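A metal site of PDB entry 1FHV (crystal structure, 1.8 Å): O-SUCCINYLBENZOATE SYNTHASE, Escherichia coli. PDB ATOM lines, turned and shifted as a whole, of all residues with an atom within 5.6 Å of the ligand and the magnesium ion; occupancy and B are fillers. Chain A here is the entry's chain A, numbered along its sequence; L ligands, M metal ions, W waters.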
ATOM      1  N   LEU A  22      -3.282   2.795 -23.450  1.00  0.00           N
ATOM      2  CA  LEU A  22      -4.709   3.032 -23.566  1.00  0.00           C
ATOM      3  C   LEU A  22      -5.133   2.815 -24.992  1.00  0.00           C
ATOM      4  O   LEU A  22      -4.639   3.568 -25.846  1.00  0.00           O
ATOM      5  CB  LEU A  22      -4.927   4.523 -23.328  1.00  0.00           C
ATOM      6  CG  LEU A  22      -5.252   4.820 -21.894  1.00  0.00           C
ATOM      7  CD1 LEU A  22      -5.579   6.295 -21.806  1.00  0.00           C
ATOM      8  CD2 LEU A  22      -6.511   4.028 -21.556  1.00  0.00           C
ATOM      9  N   LEU A  51      -9.986  12.538 -20.945  1.00  0.00           N
ATOM     10  CA  LEU A  51      -9.048  11.459 -21.266  1.00  0.00           C
ATOM     11  C   LEU A  51      -8.798  11.353 -22.787  1.00  0.00           C
ATOM     12  O   LEU A  51      -9.696  11.073 -23.580  1.00  0.00           O
ATOM     13  CB  LEU A  51      -9.651  10.159 -20.721  1.00  0.00           C
ATOM     14  CG  LEU A  51      -8.783   8.903 -20.891  1.00  0.00           C
ATOM     15  CD1 LEU A  51      -7.508   9.022 -20.030  1.00  0.00           C
ATOM     16  CD2 LEU A  51      -9.628   7.674 -20.474  1.00  0.00           C
ATOM     17  N   PHE A  54     -10.639   9.263 -25.661  1.00  0.00           N
ATOM     18  CA  PHE A  54     -11.949   8.889 -25.196  1.00  0.00           C
ATOM     19  C   PHE A  54     -12.835  10.095 -25.183  1.00  0.00           C
ATOM     20  O   PHE A  54     -13.891  10.131 -25.823  1.00  0.00           O
ATOM     21  CB  PHE A  54     -11.922   8.249 -23.815  1.00  0.00           C
ATOM     22  CG  PHE A  54     -11.266   6.888 -23.889  1.00  0.00           C
ATOM     23  CD1 PHE A  54      -9.878   6.790 -24.065  1.00  0.00           C
ATOM     24  CD2 PHE A  54     -12.028   5.726 -23.876  1.00  0.00           C
ATOM     25  CE1 PHE A  54      -9.262   5.544 -24.151  1.00  0.00           C
ATOM     26  CE2 PHE A  54     -11.433   4.469 -23.957  1.00  0.00           C
ATOM     27  CZ  PHE A  54     -10.044   4.392 -24.041  1.00  0.00           C
ATOM     28  N   LYS A 134     -11.149  -8.416 -12.246  1.00  0.00           N
ATOM     29  CA  LYS A 134     -11.262  -8.016 -13.629  1.00  0.00           C
ATOM     30  C   LYS A 134     -10.089  -8.524 -14.489  1.00  0.00           C
ATOM     31  O   LYS A 134      -8.933  -8.359 -14.120  1.00  0.00           O
ATOM     32  CB  LYS A 134     -11.373  -6.502 -13.764  1.00  0.00           C
ATOM     33  CG  LYS A 134     -11.313  -6.035 -15.215  1.00  0.00           C
ATOM     34  CD  LYS A 134     -11.452  -4.529 -15.379  1.00  0.00           C
ATOM     35  CE  LYS A 134     -12.337  -4.124 -16.552  1.00  0.00           C
ATOM     36  NZ  LYS A 134     -13.698  -4.686 -16.480  1.00  0.00           N
ATOM     37  N   LYS A 136      -8.571  -8.589 -18.559  1.00  0.00           N
ATOM     38  CA  LYS A 136      -8.728  -8.104 -19.926  1.00  0.00           C
ATOM     39  C   LYS A 136      -8.665  -9.283 -20.880  1.00  0.00           C
ATOM     40  O   LYS A 136      -7.855 -10.166 -20.657  1.00  0.00           O
ATOM     41  CB  LYS A 136      -7.649  -7.133 -20.303  1.00  0.00           C
ATOM     42  CG  LYS A 136      -7.911  -5.770 -19.721  1.00  0.00           C
ATOM     43  CD  LYS A 136      -6.721  -4.839 -19.809  1.00  0.00           C
ATOM     44  CE  LYS A 136      -6.946  -3.529 -19.075  1.00  0.00           C
ATOM     45  NZ  LYS A 136      -5.940  -2.500 -19.405  1.00  0.00           N
ATOM     46  N   ASP A 164     -13.211  -7.922 -20.033  1.00  0.00           N
ATOM     47  CA  ASP A 164     -13.347  -6.818 -20.951  1.00  0.00           C
ATOM     48  C   ASP A 164     -12.637  -7.056 -22.242  1.00  0.00           C
ATOM     49  O   ASP A 164     -11.403  -7.103 -22.250  1.00  0.00           O
ATOM     50  CB  ASP A 164     -12.903  -5.477 -20.324  1.00  0.00           C
ATOM     51  CG  ASP A 164     -13.335  -4.248 -21.142  1.00  0.00           C
ATOM     52  OD1 ASP A 164     -13.743  -4.277 -22.306  1.00  0.00           O
ATOM     53  OD2 ASP A 164     -13.138  -3.121 -20.501  1.00  0.00           O
ATOM     54  N   ASN A 166     -13.101  -5.002 -25.044  1.00  0.00           N
ATOM     55  CA  ASN A 166     -12.880  -3.800 -25.794  1.00  0.00           C
ATOM     56  C   ASN A 166     -13.222  -3.986 -27.261  1.00  0.00           C
ATOM     57  O   ASN A 166     -12.447  -3.542 -28.135  1.00  0.00           O
ATOM     58  CB  ASN A 166     -11.419  -3.302 -25.646  1.00  0.00           C
ATOM     59  CG  ASN A 166     -11.191  -2.886 -24.181  1.00  0.00           C
ATOM     60  OD1 ASN A 166     -11.811  -1.945 -23.688  1.00  0.00           O
ATOM     61  ND2 ASN A 166     -10.377  -3.626 -23.450  1.00  0.00           N
ATOM     62  N   GLU A 193     -17.488  -7.296 -20.883  1.00  0.00           N
ATOM     63  CA  GLU A 193     -17.687  -6.048 -21.595  1.00  0.00           C
ATOM     64  C   GLU A 193     -17.404  -6.116 -23.065  1.00  0.00           C
ATOM     65  O   GLU A 193     -16.311  -6.452 -23.477  1.00  0.00           O
ATOM     66  CB  GLU A 193     -16.839  -4.838 -21.047  1.00  0.00           C
ATOM     67  CG  GLU A 193     -16.943  -4.720 -19.524  1.00  0.00           C
ATOM     68  CD  GLU A 193     -16.127  -3.601 -18.952  1.00  0.00           C
ATOM     69  OE1 GLU A 193     -15.724  -3.602 -17.811  1.00  0.00           O
ATOM     70  OE2 GLU A 193     -15.894  -2.626 -19.786  1.00  0.00           O
ATOM     71  N   ASP A 216     -20.103  -0.591 -22.310  1.00  0.00           N
ATOM     72  CA  ASP A 216     -19.150   0.403 -21.785  1.00  0.00           C
ATOM     73  C   ASP A 216     -19.049   1.557 -22.778  1.00  0.00           C
ATOM     74  O   ASP A 216     -19.839   2.506 -22.739  1.00  0.00           O
ATOM     75  CB  ASP A 216     -17.773  -0.294 -21.442  1.00  0.00           C
ATOM     76  CG  ASP A 216     -16.736   0.623 -20.809  1.00  0.00           C
ATOM     77  OD1 ASP A 216     -15.603   0.331 -20.616  1.00  0.00           O
ATOM     78  OD2 ASP A 216     -17.138   1.817 -20.610  1.00  0.00           O
ATOM     79  N   VAL A 236     -21.390  -0.041 -17.780  1.00  0.00           N
ATOM     80  CA  VAL A 236     -20.169   0.573 -17.196  1.00  0.00           C
ATOM     81  C   VAL A 236     -20.246   2.068 -17.447  1.00  0.00           C
ATOM     82  O   VAL A 236     -20.163   2.572 -18.583  1.00  0.00           O
ATOM     83  CB  VAL A 236     -18.908   0.004 -17.843  1.00  0.00           C
ATOM     84  CG1 VAL A 236     -17.660   0.630 -17.192  1.00  0.00           C
ATOM     85  CG2 VAL A 236     -18.916  -1.508 -17.555  1.00  0.00           C
ATOM     86  N   LYS A 238     -18.692   5.625 -16.845  1.00  0.00           N
ATOM     87  CA  LYS A 238     -17.491   6.392 -16.572  1.00  0.00           C
ATOM     88  C   LYS A 238     -17.851   7.886 -16.470  1.00  0.00           C
ATOM     89  O   LYS A 238     -17.899   8.617 -17.471  1.00  0.00           O
ATOM     90  CB  LYS A 238     -16.491   6.162 -17.711  1.00  0.00           C
ATOM     91  CG  LYS A 238     -15.935   4.723 -17.710  1.00  0.00           C
ATOM     92  CD  LYS A 238     -14.922   4.586 -18.849  1.00  0.00           C
ATOM     93  CE  LYS A 238     -14.027   3.367 -18.735  1.00  0.00           C
ATOM     94  NZ  LYS A 238     -14.829   2.151 -18.697  1.00  0.00           N
ATOM     95  N   SER A 265     -17.053   3.491 -13.026  1.00  0.00           N
ATOM     96  CA  SER A 265     -15.757   3.147 -13.555  1.00  0.00           C
ATOM     97  C   SER A 265     -14.821   4.323 -13.815  1.00  0.00           C
ATOM     98  O   SER A 265     -15.216   5.452 -14.179  1.00  0.00           O
ATOM     99  CB  SER A 265     -16.003   2.240 -14.774  1.00  0.00           C
ATOM    100  OG  SER A 265     -14.936   2.302 -15.693  1.00  0.00           O
ATOM    101  N   SER A 266     -13.534   4.057 -13.632  1.00  0.00           N
ATOM    102  CA  SER A 266     -12.484   5.030 -13.774  1.00  0.00           C
ATOM    103  C   SER A 266     -12.175   5.453 -15.163  1.00  0.00           C
ATOM    104  O   SER A 266     -12.197   4.654 -16.092  1.00  0.00           O
ATOM    105  CB  SER A 266     -11.226   4.491 -13.130  1.00  0.00           C
ATOM    106  OG  SER A 266     -10.151   5.302 -13.612  1.00  0.00           O
ATOM    107  N   SER A 267     -11.834   6.735 -15.324  1.00  0.00           N
ATOM    108  CA  SER A 267     -11.315   7.273 -16.596  1.00  0.00           C
ATOM    109  C   SER A 267      -9.865   7.720 -16.329  1.00  0.00           C
ATOM    110  O   SER A 267      -9.385   8.738 -16.884  1.00  0.00           O
ATOM    111  CB  SER A 267     -12.127   8.456 -17.183  1.00  0.00           C
ATOM    112  OG  SER A 267     -13.470   8.039 -17.303  1.00  0.00           O
ATOM    113  N   ILE A 268      -9.202   6.993 -15.403  1.00  0.00           N
ATOM    114  CA  ILE A 268      -7.840   7.313 -15.008  1.00  0.00           C
ATOM    115  C   ILE A 268      -7.736   8.687 -14.352  1.00  0.00           C
ATOM    116  O   ILE A 268      -6.857   9.450 -14.659  1.00  0.00           O
ATOM    117  CB  ILE A 268      -6.805   7.184 -16.139  1.00  0.00           C
ATOM    118  CG1 ILE A 268      -7.114   5.973 -17.028  1.00  0.00           C
ATOM    119  CG2 ILE A 268      -5.383   7.106 -15.554  1.00  0.00           C
ATOM    120  CD1 ILE A 268      -6.110   5.796 -18.168  1.00  0.00           C
ATOM    121  N   GLY A 291     -15.160  -0.033 -10.677  1.00  0.00           N
ATOM    122  CA  GLY A 291     -13.998  -0.291 -11.527  1.00  0.00           C
ATOM    123  C   GLY A 291     -13.007   0.809 -11.394  1.00  0.00           C
ATOM    124  O   GLY A 291     -12.776   1.565 -12.332  1.00  0.00           O
ATOM    125  N   LEU A 292     -12.407   0.899 -10.206  1.00  0.00           N
ATOM    126  CA  LEU A 292     -11.510   2.025  -9.958  1.00  0.00           C
ATOM    127  C   LEU A 292     -10.038   1.677  -9.770  1.00  0.00           C
ATOM    128  O   LEU A 292      -9.279   2.466  -9.166  1.00  0.00           O
ATOM    129  CB  LEU A 292     -12.010   2.803  -8.703  1.00  0.00           C
ATOM    130  CG  LEU A 292     -13.520   3.063  -8.749  1.00  0.00           C
ATOM    131  CD1 LEU A 292     -13.910   3.801  -7.459  1.00  0.00           C
ATOM    132  CD2 LEU A 292     -13.794   3.993  -9.920  1.00  0.00           C
ATOM    133  N   ASP A 293      -9.642   0.503 -10.256  1.00  0.00           N
ATOM    134  CA  ASP A 293      -8.271   0.056 -10.034  1.00  0.00           C
ATOM    135  C   ASP A 293      -7.312   0.624 -11.020  1.00  0.00           C
ATOM    136  O   ASP A 293      -6.711  -0.097 -11.831  1.00  0.00           O
ATOM    137  CB  ASP A 293      -8.205  -1.489  -9.919  1.00  0.00           C
ATOM    138  CG  ASP A 293      -6.822  -1.932  -9.515  1.00  0.00           C
ATOM    139  OD1 ASP A 293      -6.011  -1.194  -8.999  1.00  0.00           O
ATOM    140  OD2 ASP A 293      -6.583  -3.166  -9.794  1.00  0.00           O
ATOM    141  N   THR A 294      -7.148   1.932 -10.974  1.00  0.00           N
ATOM    142  CA  THR A 294      -6.264   2.617 -11.861  1.00  0.00           C
ATOM    143  C   THR A 294      -5.251   3.533 -11.161  1.00  0.00           C
ATOM    144  O   THR A 294      -4.483   4.186 -11.830  1.00  0.00           O
ATOM    145  CB  THR A 294      -7.019   3.450 -12.916  1.00  0.00           C
ATOM    146  OG1 THR A 294      -7.805   4.421 -12.237  1.00  0.00           O
ATOM    147  CG2 THR A 294      -7.920   2.556 -13.814  1.00  0.00           C
HETATM  148  O1  LIG L   1     -12.666  -0.113 -20.374  1.00  0.00           O
HETATM  149  O2  LIG L   1     -10.644  -0.592 -20.973  1.00  0.00           O
HETATM  150  C1  LIG L   1     -11.438   0.116 -20.336  1.00  0.00           C
HETATM  151  C2  LIG L   1     -10.615   2.887 -17.919  1.00  0.00           C
HETATM  152  C3  LIG L   1     -10.242   3.922 -18.769  1.00  0.00           C
HETATM  153  C4  LIG L   1     -10.259   3.695 -20.150  1.00  0.00           C
HETATM  154  C5  LIG L   1     -10.646   2.467 -20.673  1.00  0.00           C
HETATM  155  C6  LIG L   1     -11.029   1.422 -19.825  1.00  0.00           C
HETATM  156  C7  LIG L   1     -10.998   1.666 -18.448  1.00  0.00           C
HETATM  157  C8  LIG L   1     -11.347   0.632 -17.511  1.00  0.00           C
HETATM  158  C9  LIG L   1     -11.151   1.326 -16.151  1.00  0.00           C
HETATM  159  O3  LIG L   1     -11.711  -0.536 -17.693  1.00  0.00           O
HETATM  160  C10 LIG L   1     -11.423   0.398 -14.968  1.00  0.00           C
HETATM  161  C11 LIG L   1     -12.687  -0.453 -15.060  1.00  0.00           C
HETATM  162  O4  LIG L   1     -12.682  -1.512 -14.421  1.00  0.00           O
HETATM  163  O5  LIG L   1     -13.580  -0.256 -15.904  1.00  0.00           O
HETATM  164 MG    MG M   1     -14.425  -1.377 -20.492  1.00  0.00          MG
HETATM  165  O   HOH W   1     -14.107  -1.051 -18.267  1.00  0.00           O
HETATM  166  O   HOH W   2      -9.976  -2.921 -20.773  1.00  0.00           O
HETATM  167  O   HOH W   3     -14.361  -3.658 -12.995  1.00  0.00           O
HETATM  168  O   HOH W   4     -14.986  -1.871 -22.444  1.00  0.00           O
HETATM  169  O   HOH W   5     -16.015  -2.383 -15.243  1.00  0.00           O
HETATM  170  O   HOH W   6     -10.744  -1.384 -12.083  1.00  0.00           O
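O2 of the ligand lies close to OD1 of Asn 166. OG of Ser 265 sits at hydrogen-bond distance from O5 of the ligand (2.9 Å). The side-chain amino group (NZ) of Lys 134 is in salt-bridge range of an oxygen (O4) of the ligand (3.9 Å). O5 of the ligand lies within salt-bridge range of NZ of Lys 238.
The side-chain carboxylate (OD1) of Asp 164 sits at hydrogen-bond distance from the backbone NH (N) of Asn 166 (2.9 Å). OG of Ser 266 lies within hydrogen-bond range of OG1 of Thr 294, at 2.9 Å. O of Gly 291 sits at hydrogen-bond distance from N of Ser 266, 2.9 Å away. The side-chain hydroxyl (OG) of Ser 265 is in hydrogen-bond range of the side-chain amino group (NZ) of Lys 238 (3.0 Å). The backbone NH of Ile 268 lies within hydrogen-bond range of the side-chain hydroxyl of Ser 266 (2.6 Å). The side-chain amino group (NZ) of Lys 238 lies within salt-bridge range of the side-chain carboxylate (OD2) of Asp 216 (3.0 Å). NZ of Lys 134 is in salt-bridge range of OE1 of Glu 193, 2.7 Å away.
Merely in contact with the ligand: Phe 54, Ser 266 and Gly 291. Of the 19 residues printed, 9 come within 4 Å of the ligand.
Lys 238 touches the magnesium ion. Of the 19 residues printed, 4 come within 4 Å of the magnesium ion. The nearest printed residue that does not touch the magnesium ion is Asn 166 (4.2 Å).
The side-chain carboxylate (OE2) of Glu 193 is bound to the magnesium ion, at 2.1 Å. The side-chain carboxylate (OD1) of Asp 216 binds the magnesium ion. Water W4 binds the magnesium ion (2.1 Å). The magnesium ion is bound by OD2 of Asp 164 (2.2 Å). An oxygen (O1) of the ligand binds the magnesium ion (2.2 Å). The magnesium ion is bound by water W1 (2.3 Å).
Water W4 bridges OD1 of Asp 164 (2.7 Å) and OD1 of Asn 166 (3.4 Å). Water W1 lies within hydrogen-bond range of O3 of the ligand (2.5 Å), OE1 of Glu 193 (3.1 Å) and NZ of Lys 238 (3.3 Å). Water W2 lies within hydrogen-bond range of O2 of the ligand (2.4 Å) and ND2 of Asn 166 (2.8 Å). Water W6 lies within hydrogen-bond range of N of Asp 293, O4 of the ligand and N of Leu 292. Water W5 lies within hydrogen-bond range of the side-chain carboxylate (OE1) of Glu 193, an oxygen (O5) of the ligand and the side-chain amino group (NZ) of Lys 134.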
